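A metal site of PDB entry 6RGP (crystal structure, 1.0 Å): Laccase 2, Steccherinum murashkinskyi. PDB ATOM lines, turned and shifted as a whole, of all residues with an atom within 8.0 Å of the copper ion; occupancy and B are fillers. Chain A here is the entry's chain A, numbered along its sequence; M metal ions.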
ATOM      1  N   CYS A 208     -24.887  10.837 -20.352  1.00  0.00           N
ATOM      2  CA  CYS A 208     -24.045  10.275 -19.289  1.00  0.00           C
ATOM      3  C   CYS A 208     -23.801  11.249 -18.146  1.00  0.00           C
ATOM      4  O   CYS A 208     -23.268  10.829 -17.119  1.00  0.00           O
ATOM      5  CB  CYS A 208     -22.685   9.835 -19.805  1.00  0.00           C
ATOM      6  SG  CYS A 208     -22.722   8.077 -20.283  1.00  0.00           S
ATOM      7  N   ASP A 209     -24.129  12.538 -18.316  1.00  0.00           N
ATOM      8  CA  ASP A 209     -23.784  13.510 -17.262  1.00  0.00           C
ATOM      9  C   ASP A 209     -24.631  14.765 -17.346  1.00  0.00           C
ATOM     10  O   ASP A 209     -25.518  14.951 -16.516  1.00  0.00           O
ATOM     11  CB  ASP A 209     -22.267  13.742 -17.234  1.00  0.00           C
ATOM     12  CG  ASP A 209     -21.817  14.838 -16.319  1.00  0.00           C
ATOM     13  OD1 ASP A 209     -22.600  15.494 -15.670  1.00  0.00           O
ATOM     14  OD2 ASP A 209     -20.566  15.087 -16.337  1.00  0.00           O
ATOM     15  N   PHE A 341     -18.128   8.365  -4.220  1.00  0.00           N
ATOM     16  CA  PHE A 341     -19.427   8.603  -3.621  1.00  0.00           C
ATOM     17  C   PHE A 341     -19.787   7.497  -2.655  1.00  0.00           C
ATOM     18  O   PHE A 341     -19.314   6.369  -2.735  1.00  0.00           O
ATOM     19  CB  PHE A 341     -20.499   8.665  -4.719  1.00  0.00           C
ATOM     20  CG  PHE A 341     -20.427   9.899  -5.567  1.00  0.00           C
ATOM     21  CD1 PHE A 341     -19.700   9.926  -6.739  1.00  0.00           C
ATOM     22  CD2 PHE A 341     -21.094  11.038  -5.148  1.00  0.00           C
ATOM     23  CE1 PHE A 341     -19.635  11.100  -7.493  1.00  0.00           C
ATOM     24  CE2 PHE A 341     -21.018  12.204  -5.917  1.00  0.00           C
ATOM     25  CZ  PHE A 341     -20.285  12.226  -7.083  1.00  0.00           C
ATOM     26  N   ALA A 392     -23.901  16.632  -1.832  1.00  0.00           N
ATOM     27  CA  ALA A 392     -22.710  15.955  -2.351  1.00  0.00           C
ATOM     28  C   ALA A 392     -22.217  16.674  -3.602  1.00  0.00           C
ATOM     29  O   ALA A 392     -23.053  17.030  -4.471  1.00  0.00           O
ATOM     30  CB  ALA A 392     -23.024  14.502  -2.677  1.00  0.00           C
ATOM     31  N   ALA A 393     -20.894  16.817  -3.739  1.00  0.00           N
ATOM     32  CA  ALA A 393     -20.302  17.441  -4.899  1.00  0.00           C
ATOM     33  C   ALA A 393     -20.762  16.814  -6.203  1.00  0.00           C
ATOM     34  O   ALA A 393     -21.151  15.647  -6.270  1.00  0.00           O
ATOM     35  CB  ALA A 393     -18.785  17.355  -4.768  1.00  0.00           C
ATOM     36  N   GLY A 394     -20.663  17.618  -7.253  1.00  0.00           N
ATOM     37  CA  GLY A 394     -20.973  17.166  -8.589  1.00  0.00           C
ATOM     38  C   GLY A 394     -22.465  17.242  -8.935  1.00  0.00           C
ATOM     39  O   GLY A 394     -22.867  16.673  -9.926  1.00  0.00           O
ATOM     40  N   GLY A 395     -23.245  17.933  -8.116  1.00  0.00           N
ATOM     41  CA  GLY A 395     -24.692  18.023  -8.361  1.00  0.00           C
ATOM     42  C   GLY A 395     -24.997  18.966  -9.523  1.00  0.00           C
ATOM     43  O   GLY A 395     -24.114  19.649 -10.051  1.00  0.00           O
ATOM     44  N   PRO A 396     -26.267  19.034  -9.913  1.00  0.00           N
ATOM     45  CA  PRO A 396     -27.408  18.349  -9.296  1.00  0.00           C
ATOM     46  C   PRO A 396     -27.483  16.892  -9.787  1.00  0.00           C
ATOM     47  O   PRO A 396     -27.383  16.600 -10.980  1.00  0.00           O
ATOM     48  CB  PRO A 396     -28.599  19.154  -9.759  1.00  0.00           C
ATOM     49  CG  PRO A 396     -28.155  19.769 -11.054  1.00  0.00           C
ATOM     50  CD  PRO A 396     -26.702  20.004 -10.914  1.00  0.00           C
ATOM     51  N   HIS A 397     -27.656  15.975  -8.820  1.00  0.00           N
ATOM     52  CA  HIS A 397     -27.625  14.548  -9.110  1.00  0.00           C
ATOM     53  C   HIS A 397     -29.023  14.041  -9.479  1.00  0.00           C
ATOM     54  O   HIS A 397     -29.940  14.136  -8.674  1.00  0.00           O
ATOM     55  CB  HIS A 397     -27.139  13.777  -7.889  1.00  0.00           C
ATOM     56  CG  HIS A 397     -25.777  14.169  -7.444  1.00  0.00           C
ATOM     57  ND1 HIS A 397     -24.630  13.763  -8.110  1.00  0.00           N
ATOM     58  CD2 HIS A 397     -25.398  14.938  -6.389  1.00  0.00           C
ATOM     59  CE1 HIS A 397     -23.607  14.324  -7.471  1.00  0.00           C
ATOM     60  NE2 HIS A 397     -24.030  15.035  -6.445  1.00  0.00           N
ATOM     61  N   PRO A 398     -29.170  13.408 -10.671  1.00  0.00           N
ATOM     62  CA  PRO A 398     -30.444  12.807 -11.037  1.00  0.00           C
ATOM     63  C   PRO A 398     -30.512  11.348 -10.570  1.00  0.00           C
ATOM     64  O   PRO A 398     -29.910  10.467 -11.171  1.00  0.00           O
ATOM     65  CB  PRO A 398     -30.437  12.925 -12.553  1.00  0.00           C
ATOM     66  CG  PRO A 398     -28.987  12.820 -12.947  1.00  0.00           C
ATOM     67  CD  PRO A 398     -28.229  13.416 -11.793  1.00  0.00           C
ATOM     68  N   PHE A 399     -31.251  11.103  -9.515  1.00  0.00           N
ATOM     69  CA  PHE A 399     -31.402   9.765  -8.971  1.00  0.00           C
ATOM     70  C   PHE A 399     -32.501   8.998  -9.671  1.00  0.00           C
ATOM     71  O   PHE A 399     -33.573   9.522  -9.944  1.00  0.00           O
ATOM     72  CB  PHE A 399     -31.624   9.780  -7.436  1.00  0.00           C
ATOM     73  CG  PHE A 399     -30.339   9.659  -6.664  1.00  0.00           C
ATOM     74  CD1 PHE A 399     -29.423  10.701  -6.632  1.00  0.00           C
ATOM     75  CD2 PHE A 399     -29.983   8.458  -6.057  1.00  0.00           C
ATOM     76  CE1 PHE A 399     -28.179  10.536  -5.997  1.00  0.00           C
ATOM     77  CE2 PHE A 399     -28.754   8.301  -5.449  1.00  0.00           C
ATOM     78  CZ  PHE A 399     -27.865   9.325  -5.414  1.00  0.00           C
ATOM     79  N   ILE A 430     -32.121  15.685  -7.432  1.00  0.00           N
ATOM     80  CA  ILE A 430     -32.191  15.928  -5.993  1.00  0.00           C
ATOM     81  C   ILE A 430     -31.795  17.343  -5.617  1.00  0.00           C
ATOM     82  O   ILE A 430     -31.860  17.730  -4.451  1.00  0.00           O
ATOM     83  CB  ILE A 430     -31.470  14.861  -5.182  1.00  0.00           C
ATOM     84  CG1 ILE A 430     -29.958  14.953  -5.308  1.00  0.00           C
ATOM     85  CG2 ILE A 430     -32.002  13.467  -5.531  1.00  0.00           C
ATOM     86  CD1 ILE A 430     -29.204  14.068  -4.346  1.00  0.00           C
ATOM     87  N   HIS A 452     -29.626   4.672  -8.016  1.00  0.00           N
ATOM     88  CA  HIS A 452     -28.337   5.287  -8.269  1.00  0.00           C
ATOM     89  C   HIS A 452     -28.463   6.621  -8.922  1.00  0.00           C
ATOM     90  O   HIS A 452     -29.451   6.939  -9.569  1.00  0.00           O
ATOM     91  CB  HIS A 452     -27.462   4.325  -9.130  1.00  0.00           C
ATOM     92  CG  HIS A 452     -27.983   4.059 -10.497  1.00  0.00           C
ATOM     93  ND1 HIS A 452     -27.713   4.880 -11.571  1.00  0.00           N
ATOM     94  CD2 HIS A 452     -28.737   3.054 -10.993  1.00  0.00           C
ATOM     95  CE1 HIS A 452     -28.294   4.387 -12.659  1.00  0.00           C
ATOM     96  NE2 HIS A 452     -28.938   3.263 -12.354  1.00  0.00           N
ATOM     97  N   CYS A 453     -27.380   7.402  -8.796  1.00  0.00           N
ATOM     98  CA  CYS A 453     -27.262   8.609  -9.598  1.00  0.00           C
ATOM     99  C   CYS A 453     -27.051   8.211 -11.055  1.00  0.00           C
ATOM    100  O   CYS A 453     -26.280   7.289 -11.359  1.00  0.00           O
ATOM    101  CB  CYS A 453     -26.077   9.446  -9.127  1.00  0.00           C
ATOM    102  SG  CYS A 453     -25.984  10.982 -10.109  1.00  0.00           S
ATOM    103  N   HIS A 454     -27.733   8.881 -11.986  1.00  0.00           N
ATOM    104  CA  HIS A 454     -27.660   8.578 -13.402  1.00  0.00           C
ATOM    105  C   HIS A 454     -26.609   9.361 -14.147  1.00  0.00           C
ATOM    106  O   HIS A 454     -26.485   9.208 -15.358  1.00  0.00           O
ATOM    107  CB  HIS A 454     -29.029   8.702 -14.089  1.00  0.00           C
ATOM    108  CG  HIS A 454     -29.270   7.614 -15.116  1.00  0.00           C
ATOM    109  ND1 HIS A 454     -28.529   7.454 -16.245  1.00  0.00           N
ATOM    110  CD2 HIS A 454     -30.177   6.601 -15.157  1.00  0.00           C
ATOM    111  CE1 HIS A 454     -28.974   6.397 -16.926  1.00  0.00           C
ATOM    112  NE2 HIS A 454     -30.002   5.854 -16.293  1.00  0.00           N
ATOM    113  N   ILE A 455     -25.783  10.154 -13.449  1.00  0.00           N
ATOM    114  CA  ILE A 455     -24.528  10.634 -14.025  1.00  0.00           C
ATOM    115  C   ILE A 455     -23.612   9.425 -13.984  1.00  0.00           C
ATOM    116  O   ILE A 455     -23.232   8.932 -12.891  1.00  0.00           O
ATOM    117  CB  ILE A 455     -23.998  11.857 -13.268  1.00  0.00           C
ATOM    118  CG1 ILE A 455     -24.960  13.027 -13.426  1.00  0.00           C
ATOM    119  CG2 ILE A 455     -22.578  12.187 -13.730  1.00  0.00           C
ATOM    120  CD1 ILE A 455     -24.727  14.175 -12.462  1.00  0.00           C
ATOM    121  N   ASP A 456     -23.271   8.878 -15.153  1.00  0.00           N
ATOM    122  CA  ASP A 456     -22.638   7.575 -15.190  1.00  0.00           C
ATOM    123  C   ASP A 456     -21.289   7.561 -14.510  1.00  0.00           C
ATOM    124  O   ASP A 456     -20.865   6.566 -13.927  1.00  0.00           O
ATOM    125  CB  ASP A 456     -22.591   7.058 -16.630  1.00  0.00           C
ATOM    126  CG  ASP A 456     -22.746   5.537 -16.772  1.00  0.00           C
ATOM    127  OD1 ASP A 456     -23.506   4.987 -15.952  1.00  0.00           O
ATOM    128  OD2 ASP A 456     -22.169   4.995 -17.716  1.00  0.00           O
ATOM    129  N   TRP A 457     -20.577   8.694 -14.587  1.00  0.00           N
ATOM    130  CA  TRP A 457     -19.288   8.824 -13.947  1.00  0.00           C
ATOM    131  C   TRP A 457     -19.443   8.686 -12.417  1.00  0.00           C
ATOM    132  O   TRP A 457     -18.546   8.215 -11.723  1.00  0.00           O
ATOM    133  CB  TRP A 457     -18.626  10.173 -14.306  1.00  0.00           C
ATOM    134  CG  TRP A 457     -18.685  10.445 -15.803  1.00  0.00           C
ATOM    135  CD1 TRP A 457     -19.417  11.429 -16.392  1.00  0.00           C
ATOM    136  CD2 TRP A 457     -18.071   9.703 -16.840  1.00  0.00           C
ATOM    137  NE1 TRP A 457     -19.275  11.373 -17.748  1.00  0.00           N
ATOM    138  CE2 TRP A 457     -18.455  10.321 -18.069  1.00  0.00           C
ATOM    139  CE3 TRP A 457     -17.184   8.627 -16.890  1.00  0.00           C
ATOM    140  CZ2 TRP A 457     -18.007   9.841 -19.307  1.00  0.00           C
ATOM    141  CZ3 TRP A 457     -16.767   8.184 -18.090  1.00  0.00           C
ATOM    142  CH2 TRP A 457     -17.171   8.769 -19.288  1.00  0.00           C
ATOM    143  N   HIS A 458     -20.579   9.136 -11.872  1.00  0.00           N
ATOM    144  CA  HIS A 458     -20.850   9.055 -10.438  1.00  0.00           C
ATOM    145  C   HIS A 458     -21.256   7.635 -10.024  1.00  0.00           C
ATOM    146  O   HIS A 458     -20.850   7.159  -8.963  1.00  0.00           O
ATOM    147  CB  HIS A 458     -21.943  10.055 -10.026  1.00  0.00           C
ATOM    148  CG  HIS A 458     -21.569  11.471 -10.287  1.00  0.00           C
ATOM    149  ND1 HIS A 458     -22.486  12.488 -10.027  1.00  0.00           N
ATOM    150  CD2 HIS A 458     -20.426  12.023 -10.739  1.00  0.00           C
ATOM    151  CE1 HIS A 458     -21.861  13.624 -10.338  1.00  0.00           C
ATOM    152  NE2 HIS A 458     -20.625  13.382 -10.767  1.00  0.00           N
ATOM    153  N   LEU A 459     -22.063   6.976 -10.861  1.00  0.00           N
ATOM    154  CA  LEU A 459     -22.352   5.562 -10.622  1.00  0.00           C
ATOM    155  C   LEU A 459     -21.056   4.763 -10.566  1.00  0.00           C
ATOM    156  O   LEU A 459     -20.854   3.941  -9.658  1.00  0.00           O
ATOM    157  CB  LEU A 459     -23.280   5.036 -11.704  1.00  0.00           C
ATOM    158  CG  LEU A 459     -23.518   3.530 -11.739  1.00  0.00           C
ATOM    159  CD1 LEU A 459     -24.049   3.012 -10.409  1.00  0.00           C
ATOM    160  CD2 LEU A 459     -24.397   3.135 -12.885  1.00  0.00           C
ATOM    161  N   PHE A 463     -21.934   5.761  -6.509  1.00  0.00           N
ATOM    162  CA  PHE A 463     -23.120   6.471  -5.991  1.00  0.00           C
ATOM    163  C   PHE A 463     -24.388   5.634  -6.241  1.00  0.00           C
ATOM    164  O   PHE A 463     -25.223   5.966  -7.095  1.00  0.00           O
ATOM    165  CB  PHE A 463     -23.232   7.845  -6.603  1.00  0.00           C
ATOM    166  CG  PHE A 463     -23.836   8.930  -5.728  1.00  0.00           C
ATOM    167  CD1 PHE A 463     -24.054   8.796  -4.362  1.00  0.00           C
ATOM    168  CD2 PHE A 463     -24.109  10.162  -6.308  1.00  0.00           C
ATOM    169  CE1 PHE A 463     -24.499   9.863  -3.594  1.00  0.00           C
ATOM    170  CE2 PHE A 463     -24.561  11.232  -5.547  1.00  0.00           C
ATOM    171  CZ  PHE A 463     -24.734  11.091  -4.199  1.00  0.00           C
HETATM  172 CU    CU M   1     -24.381  12.277  -9.450  1.00  0.00          CU
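The backbone carbonyl oxygen (O) of His 458 is in hydrogen-bond range of the backbone NH (N) of Phe 463. A ring nitrogen (NE2) of His 397 lies within hydrogen-bond range of the backbone carbonyl oxygen of Ala 393 (2.9 Å). N of Gly 395 sits at hydrogen-bond distance from NE2 of His 397, at 3.4 Å. O of Ala 392 lies within hydrogen-bond range of NE2 of His 397, at 3.0 Å. O of His 397 sits at hydrogen-bond distance from N of Ile 430, at 2.9 Å. SG of Cys 453 sits close to N of Ile 455 (3.4 Å). N of Cys 453 lies within hydrogen-bond range of O of Phe 463 (3.1 Å).
Residues that only touch the copper ion: Ile 455 (3.6 Å) and Phe 463 (3.8 Å). Five residues have an atom within 4 Å of the copper ion: His 397, Cys 453, Ile 455, His 458 and Phe 463. Along chain A the residues within 4 Å of the copper ion span positions 397 to 463.
ND1 of His 458 is bound to the copper ion (2.0 Å). A ring nitrogen (ND1) of His 397 binds the copper ion, at 2.0 Å. The side-chain sulfur (SG) of Cys 453 binds the copper ion (2.2 Å).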
